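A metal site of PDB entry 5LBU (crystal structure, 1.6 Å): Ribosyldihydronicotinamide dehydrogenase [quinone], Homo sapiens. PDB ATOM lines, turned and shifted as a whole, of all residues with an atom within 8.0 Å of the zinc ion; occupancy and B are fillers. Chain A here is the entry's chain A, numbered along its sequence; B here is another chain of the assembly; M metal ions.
NE2 of His 174 sits at hydrogen-bond distance from O of Val 161 of chain B. O of Gln 173 sits close to SG of Cys 223, at 3.7 Å. The backbone carbonyl oxygen of Gln 173 lies within hydrogen-bond range of the backbone NH of His 178. OD1 of Asp 134 lies within hydrogen-bond range of NE2 of His 178 (2.6 Å). The side-chain hydroxyl (OH) of Tyr 133 lies close to a ring nitrogen (NE2) of His 174. The backbone carbonyl oxygen (O) of His 174 sits at hydrogen-bond distance from the backbone NH (N) of Phe 179, at 3.1 Å.
Within 4 Å of the zinc ion: His 174, His 178 and Cys 223. The nearest printed residue that does not touch the zinc ion is Thr 224 (4.1 Å).
The zinc ion is bound by ND1 of His 174 (2.1 Å), O of Cys 223 (2.2 Å), ND1 of His 178 (2.2 Å) and SG of Cys 223 (2.2 Å).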
ATOM      1  N   TYR A 133       4.767 -13.011  -3.242  1.00  0.00           N
ATOM      2  CA  TYR A 133       5.754 -14.056  -3.566  1.00  0.00           C
ATOM      3  C   TYR A 133       7.125 -13.684  -2.994  1.00  0.00           C
ATOM      4  O   TYR A 133       7.181 -13.341  -1.819  1.00  0.00           O
ATOM      5  CB  TYR A 133       5.697 -14.473  -5.048  1.00  0.00           C
ATOM      6  CG  TYR A 133       4.422 -15.237  -5.344  1.00  0.00           C
ATOM      7  CD1 TYR A 133       4.129 -16.428  -4.659  1.00  0.00           C
ATOM      8  CD2 TYR A 133       3.492 -14.764  -6.265  1.00  0.00           C
ATOM      9  CE1 TYR A 133       2.952 -17.125  -4.892  1.00  0.00           C
ATOM     10  CE2 TYR A 133       2.306 -15.452  -6.505  1.00  0.00           C
ATOM     11  CZ  TYR A 133       2.050 -16.633  -5.822  1.00  0.00           C
ATOM     12  OH  TYR A 133       0.864 -17.301  -6.064  1.00  0.00           O
ATOM     13  N   ASP A 134       8.214 -13.672  -3.763  1.00  0.00           N
ATOM     14  CA  ASP A 134       9.545 -13.370  -3.194  1.00  0.00           C
ATOM     15  C   ASP A 134       9.630 -11.987  -2.518  1.00  0.00           C
ATOM     16  O   ASP A 134      10.407 -11.834  -1.583  1.00  0.00           O
ATOM     17  CB  ASP A 134      10.670 -13.509  -4.228  1.00  0.00           C
ATOM     18  CG  ASP A 134      10.964 -14.971  -4.613  1.00  0.00           C
ATOM     19  OD1 ASP A 134      10.341 -15.916  -4.081  1.00  0.00           O
ATOM     20  OD2 ASP A 134      11.854 -15.171  -5.476  1.00  0.00           O
ATOM     21  N   TRP A 170       0.483 -27.464  -2.382  1.00  0.00           N
ATOM     22  CA  TRP A 170       0.539 -26.270  -3.220  1.00  0.00           C
ATOM     23  C   TRP A 170      -0.216 -25.042  -2.697  1.00  0.00           C
ATOM     24  O   TRP A 170       0.382 -23.967  -2.605  1.00  0.00           O
ATOM     25  CB  TRP A 170       0.107 -26.631  -4.662  1.00  0.00           C
ATOM     26  CG  TRP A 170      -0.081 -25.487  -5.593  1.00  0.00           C
ATOM     27  CD1 TRP A 170      -1.266 -24.946  -6.006  1.00  0.00           C
ATOM     28  CD2 TRP A 170       0.949 -24.761  -6.279  1.00  0.00           C
ATOM     29  NE1 TRP A 170      -1.025 -23.920  -6.903  1.00  0.00           N
ATOM     30  CE2 TRP A 170       0.323 -23.795  -7.098  1.00  0.00           C
ATOM     31  CE3 TRP A 170       2.336 -24.858  -6.298  1.00  0.00           C
ATOM     32  CZ2 TRP A 170       1.047 -22.912  -7.913  1.00  0.00           C
ATOM     33  CZ3 TRP A 170       3.060 -23.974  -7.113  1.00  0.00           C
ATOM     34  CH2 TRP A 170       2.410 -23.015  -7.911  1.00  0.00           C
ATOM     35  N   LEU A 172      -0.982 -24.294   0.292  1.00  0.00           N
ATOM     36  CA  LEU A 172      -0.391 -23.880   1.577  1.00  0.00           C
ATOM     37  C   LEU A 172       0.999 -23.299   1.401  1.00  0.00           C
ATOM     38  O   LEU A 172       1.270 -22.168   1.807  1.00  0.00           O
ATOM     39  CB  LEU A 172      -0.357 -25.071   2.538  1.00  0.00           C
ATOM     40  CG  LEU A 172      -1.749 -25.659   2.818  1.00  0.00           C
ATOM     41  CD1 LEU A 172      -1.635 -26.988   3.539  1.00  0.00           C
ATOM     42  CD2 LEU A 172      -2.615 -24.675   3.595  1.00  0.00           C
ATOM     43  N   GLN A 173       1.884 -24.075   0.787  1.00  0.00           N
ATOM     44  CA  GLN A 173       3.295 -23.663   0.631  1.00  0.00           C
ATOM     45  C   GLN A 173       3.412 -22.507  -0.365  1.00  0.00           C
ATOM     46  O   GLN A 173       4.050 -21.480  -0.079  1.00  0.00           O
ATOM     47  CB  GLN A 173       4.156 -24.860   0.203  1.00  0.00           C
ATOM     48  CG  GLN A 173       4.227 -25.949   1.268  1.00  0.00           C
ATOM     49  CD  GLN A 173       5.262 -27.045   1.025  1.00  0.00           C
ATOM     50  OE1 GLN A 173       5.792 -27.606   1.964  1.00  0.00           O
ATOM     51  NE2 GLN A 173       5.530 -27.367  -0.229  1.00  0.00           N
ATOM     52  N   HIS A 174       2.761 -22.634  -1.519  1.00  0.00           N
ATOM     53  CA  HIS A 174       2.869 -21.604  -2.565  1.00  0.00           C
ATOM     54  C   HIS A 174       1.844 -20.489  -2.423  1.00  0.00           C
ATOM     55  O   HIS A 174       2.204 -19.292  -2.334  1.00  0.00           O
ATOM     56  CB  HIS A 174       2.770 -22.232  -3.954  1.00  0.00           C
ATOM     57  CG  HIS A 174       2.994 -21.249  -5.055  1.00  0.00           C
ATOM     58  ND1 HIS A 174       4.253 -20.819  -5.408  1.00  0.00           N
ATOM     59  CD2 HIS A 174       2.131 -20.591  -5.852  1.00  0.00           C
ATOM     60  CE1 HIS A 174       4.156 -19.954  -6.405  1.00  0.00           C
ATOM     61  NE2 HIS A 174       2.875 -19.801  -6.691  1.00  0.00           N
ATOM     62  N   GLY A 175       0.574 -20.869  -2.433  1.00  0.00           N
ATOM     63  CA  GLY A 175      -0.517 -19.909  -2.418  1.00  0.00           C
ATOM     64  C   GLY A 175      -0.590 -19.043  -1.157  1.00  0.00           C
ATOM     65  O   GLY A 175      -1.103 -17.941  -1.213  1.00  0.00           O
ATOM     66  N   THR A 176      -0.064 -19.543  -0.041  1.00  0.00           N
ATOM     67  CA  THR A 176      -0.098 -18.846   1.250  1.00  0.00           C
ATOM     68  C   THR A 176       1.303 -18.416   1.705  1.00  0.00           C
ATOM     69  O   THR A 176       1.601 -17.221   1.782  1.00  0.00           O
ATOM     70  CB  THR A 176      -0.808 -19.711   2.317  1.00  0.00           C
ATOM     71  OG1 THR A 176      -2.056 -20.210   1.785  1.00  0.00           O
ATOM     72  CG2 THR A 176      -1.098 -18.913   3.597  1.00  0.00           C
ATOM     73  N   LEU A 177       2.164 -19.389   2.023  1.00  0.00           N
ATOM     74  CA  LEU A 177       3.451 -19.091   2.647  1.00  0.00           C
ATOM     75  C   LEU A 177       4.400 -18.334   1.699  1.00  0.00           C
ATOM     76  O   LEU A 177       4.875 -17.223   2.018  1.00  0.00           O
ATOM     77  CB  LEU A 177       4.063 -20.386   3.227  1.00  0.00           C
ATOM     78  CG  LEU A 177       3.212 -21.067   4.318  1.00  0.00           C
ATOM     79  CD1 LEU A 177       3.783 -22.423   4.717  1.00  0.00           C
ATOM     80  CD2 LEU A 177       3.042 -20.175   5.542  1.00  0.00           C
ATOM     81  N   HIS A 178       4.650 -18.899   0.521  1.00  0.00           N
ATOM     82  CA  HIS A 178       5.473 -18.208  -0.482  1.00  0.00           C
ATOM     83  C   HIS A 178       4.841 -16.858  -0.835  1.00  0.00           C
ATOM     84  O   HIS A 178       5.533 -15.854  -0.935  1.00  0.00           O
ATOM     85  CB  HIS A 178       5.681 -19.083  -1.732  1.00  0.00           C
ATOM     86  CG  HIS A 178       6.665 -18.542  -2.716  1.00  0.00           C
ATOM     87  ND1 HIS A 178       6.804 -19.057  -3.989  1.00  0.00           N
ATOM     88  CD2 HIS A 178       7.525 -17.500  -2.652  1.00  0.00           C
ATOM     89  CE1 HIS A 178       7.738 -18.388  -4.644  1.00  0.00           C
ATOM     90  NE2 HIS A 178       8.185 -17.434  -3.844  1.00  0.00           N
ATOM     91  N   PHE A 179       3.513 -16.827  -0.949  1.00  0.00           N
ATOM     92  CA  PHE A 179       2.842 -15.579  -1.325  1.00  0.00           C
ATOM     93  C   PHE A 179       3.179 -14.428  -0.379  1.00  0.00           C
ATOM     94  O   PHE A 179       3.356 -13.290  -0.823  1.00  0.00           O
ATOM     95  CB  PHE A 179       1.330 -15.767  -1.418  1.00  0.00           C
ATOM     96  CG  PHE A 179       0.611 -14.582  -2.002  1.00  0.00           C
ATOM     97  CD1 PHE A 179       0.436 -14.474  -3.379  1.00  0.00           C
ATOM     98  CD2 PHE A 179       0.092 -13.594  -1.183  1.00  0.00           C
ATOM     99  CE1 PHE A 179      -0.240 -13.396  -3.926  1.00  0.00           C
ATOM    100  CE2 PHE A 179      -0.598 -12.516  -1.726  1.00  0.00           C
ATOM    101  CZ  PHE A 179      -0.750 -12.418  -3.101  1.00  0.00           C
ATOM    102  N   PHE A 182       7.514 -15.904   2.722  1.00  0.00           N
ATOM    103  CA  PHE A 182       8.246 -16.897   3.479  1.00  0.00           C
ATOM    104  C   PHE A 182       9.087 -17.720   2.529  1.00  0.00           C
ATOM    105  O   PHE A 182       8.750 -17.868   1.377  1.00  0.00           O
ATOM    106  CB  PHE A 182       7.301 -17.899   4.130  1.00  0.00           C
ATOM    107  CG  PHE A 182       6.609 -17.408   5.358  1.00  0.00           C
ATOM    108  CD1 PHE A 182       7.270 -17.326   6.558  1.00  0.00           C
ATOM    109  CD2 PHE A 182       5.269 -17.075   5.331  1.00  0.00           C
ATOM    110  CE1 PHE A 182       6.633 -16.895   7.697  1.00  0.00           C
ATOM    111  CE2 PHE A 182       4.620 -16.656   6.453  1.00  0.00           C
ATOM    112  CZ  PHE A 182       5.300 -16.556   7.639  1.00  0.00           C
ATOM    113  N   VAL A 184      10.199 -21.450   2.221  1.00  0.00           N
ATOM    114  CA  VAL A 184       9.621 -22.646   2.762  1.00  0.00           C
ATOM    115  C   VAL A 184      10.579 -23.807   2.935  1.00  0.00           C
ATOM    116  O   VAL A 184      11.193 -24.235   1.993  1.00  0.00           O
ATOM    117  CB  VAL A 184       8.477 -23.129   1.834  1.00  0.00           C
ATOM    118  CG1 VAL A 184       7.849 -24.420   2.332  1.00  0.00           C
ATOM    119  CG2 VAL A 184       7.442 -22.037   1.680  1.00  0.00           C
ATOM    120  N   ILE A 221      13.062 -25.066   0.100  1.00  0.00           N
ATOM    121  CA  ILE A 221      12.732 -25.700  -1.169  1.00  0.00           C
ATOM    122  C   ILE A 221      12.595 -24.644  -2.257  1.00  0.00           C
ATOM    123  O   ILE A 221      12.353 -23.472  -1.950  1.00  0.00           O
ATOM    124  CB  ILE A 221      11.427 -26.535  -1.112  1.00  0.00           C
ATOM    125  CG1 ILE A 221      10.191 -25.658  -0.858  1.00  0.00           C
ATOM    126  CG2 ILE A 221      11.548 -27.625  -0.052  1.00  0.00           C
ATOM    127  CD1 ILE A 221       8.880 -26.332  -1.244  1.00  0.00           C
ATOM    128  N   PRO A 222      12.761 -25.038  -3.528  1.00  0.00           N
ATOM    129  CA  PRO A 222      12.360 -24.141  -4.603  1.00  0.00           C
ATOM    130  C   PRO A 222      10.836 -24.241  -4.725  1.00  0.00           C
ATOM    131  O   PRO A 222      10.314 -25.263  -5.152  1.00  0.00           O
ATOM    132  CB  PRO A 222      13.088 -24.721  -5.823  1.00  0.00           C
ATOM    133  CG  PRO A 222      13.250 -26.178  -5.527  1.00  0.00           C
ATOM    134  CD  PRO A 222      13.188 -26.353  -4.036  1.00  0.00           C
ATOM    135  N   CYS A 223      10.122 -23.212  -4.272  1.00  0.00           N
ATOM    136  CA  CYS A 223       8.662 -23.305  -4.146  1.00  0.00           C
ATOM    137  C   CYS A 223       8.039 -22.930  -5.481  1.00  0.00           C
ATOM    138  O   CYS A 223       7.528 -21.816  -5.700  1.00  0.00           O
ATOM    139  CB  CYS A 223       8.141 -22.458  -2.974  1.00  0.00           C
ATOM    140  SG  CYS A 223       6.349 -22.635  -2.709  1.00  0.00           S
ATOM    141  N   THR A 224       8.111 -23.877  -6.394  1.00  0.00           N
ATOM    142  CA  THR A 224       7.729 -23.667  -7.766  1.00  0.00           C
ATOM    143  C   THR A 224       6.638 -24.649  -8.115  1.00  0.00           C
ATOM    144  O   THR A 224       6.488 -25.679  -7.433  1.00  0.00           O
ATOM    145  CB  THR A 224       8.929 -23.885  -8.700  1.00  0.00           C
ATOM    146  OG1 THR A 224       9.362 -25.248  -8.639  1.00  0.00           O
ATOM    147  CG2 THR A 224      10.077 -22.951  -8.323  1.00  0.00           C
ATOM    148  N   ALA A 225       5.907 -24.344  -9.179  1.00  0.00           N
ATOM    149  CA  ALA A 225       4.975 -25.302  -9.764  1.00  0.00           C
ATOM    150  C   ALA A 225       5.680 -26.626 -10.071  1.00  0.00           C
ATOM    151  O   ALA A 225       5.145 -27.699  -9.777  1.00  0.00           O
ATOM    152  CB  ALA A 225       4.323 -24.725 -11.010  1.00  0.00           C
ATOM    153  N   TRP A 227       8.328 -27.986  -8.580  1.00  0.00           N
ATOM    154  CA  TRP A 227       8.566 -28.765  -7.358  1.00  0.00           C
ATOM    155  C   TRP A 227       7.323 -29.552  -6.955  1.00  0.00           C
ATOM    156  O   TRP A 227       7.416 -30.713  -6.534  1.00  0.00           O
ATOM    157  CB  TRP A 227       9.015 -27.872  -6.200  1.00  0.00           C
ATOM    158  CG  TRP A 227       9.464 -28.623  -4.984  1.00  0.00           C
ATOM    159  CD1 TRP A 227      10.744 -28.994  -4.673  1.00  0.00           C
ATOM    160  CD2 TRP A 227       8.644 -29.085  -3.911  1.00  0.00           C
ATOM    161  NE1 TRP A 227      10.759 -29.666  -3.478  1.00  0.00           N
ATOM    162  CE2 TRP A 227       9.492 -29.727  -2.973  1.00  0.00           C
ATOM    163  CE3 TRP A 227       7.279 -29.020  -3.630  1.00  0.00           C
ATOM    164  CZ2 TRP A 227       9.015 -30.299  -1.801  1.00  0.00           C
ATOM    165  CZ3 TRP A 227       6.797 -29.591  -2.449  1.00  0.00           C
ATOM    166  CH2 TRP A 227       7.671 -30.218  -1.556  1.00  0.00           C
ATOM    167  N   HIS A 228       6.163 -28.920  -7.084  1.00  0.00           N
ATOM    168  CA  HIS A 228       4.923 -29.517  -6.607  1.00  0.00           C
ATOM    169  C   HIS A 228       4.348 -30.548  -7.555  1.00  0.00           C
ATOM    170  O   HIS A 228       3.838 -31.563  -7.112  1.00  0.00           O
ATOM    171  CB  HIS A 228       3.893 -28.445  -6.311  1.00  0.00           C
ATOM    172  CG  HIS A 228       4.222 -27.626  -5.099  1.00  0.00           C
ATOM    173  ND1 HIS A 228       5.071 -26.546  -5.138  1.00  0.00           N
ATOM    174  CD2 HIS A 228       3.788 -27.723  -3.815  1.00  0.00           C
ATOM    175  CE1 HIS A 228       5.169 -26.020  -3.936  1.00  0.00           C
ATOM    176  NE2 HIS A 228       4.403 -26.710  -3.110  1.00  0.00           N
ATOM    177  N   VAL B 161       2.061 -15.998 -12.207  1.00  0.00           N
ATOM    178  CA  VAL B 161       2.596 -16.110 -10.850  1.00  0.00           C
ATOM    179  C   VAL B 161       1.870 -17.103  -9.941  1.00  0.00           C
ATOM    180  O   VAL B 161       2.469 -17.646  -9.022  1.00  0.00           O
ATOM    181  CB  VAL B 161       2.705 -14.732 -10.135  1.00  0.00           C
ATOM    182  CG1 VAL B 161       3.778 -13.884 -10.809  1.00  0.00           C
ATOM    183  CG2 VAL B 161       1.372 -14.000 -10.097  1.00  0.00           C
HETATM  184 ZN    ZN M   1       6.051 -21.090  -4.287  1.00  0.00          ZN
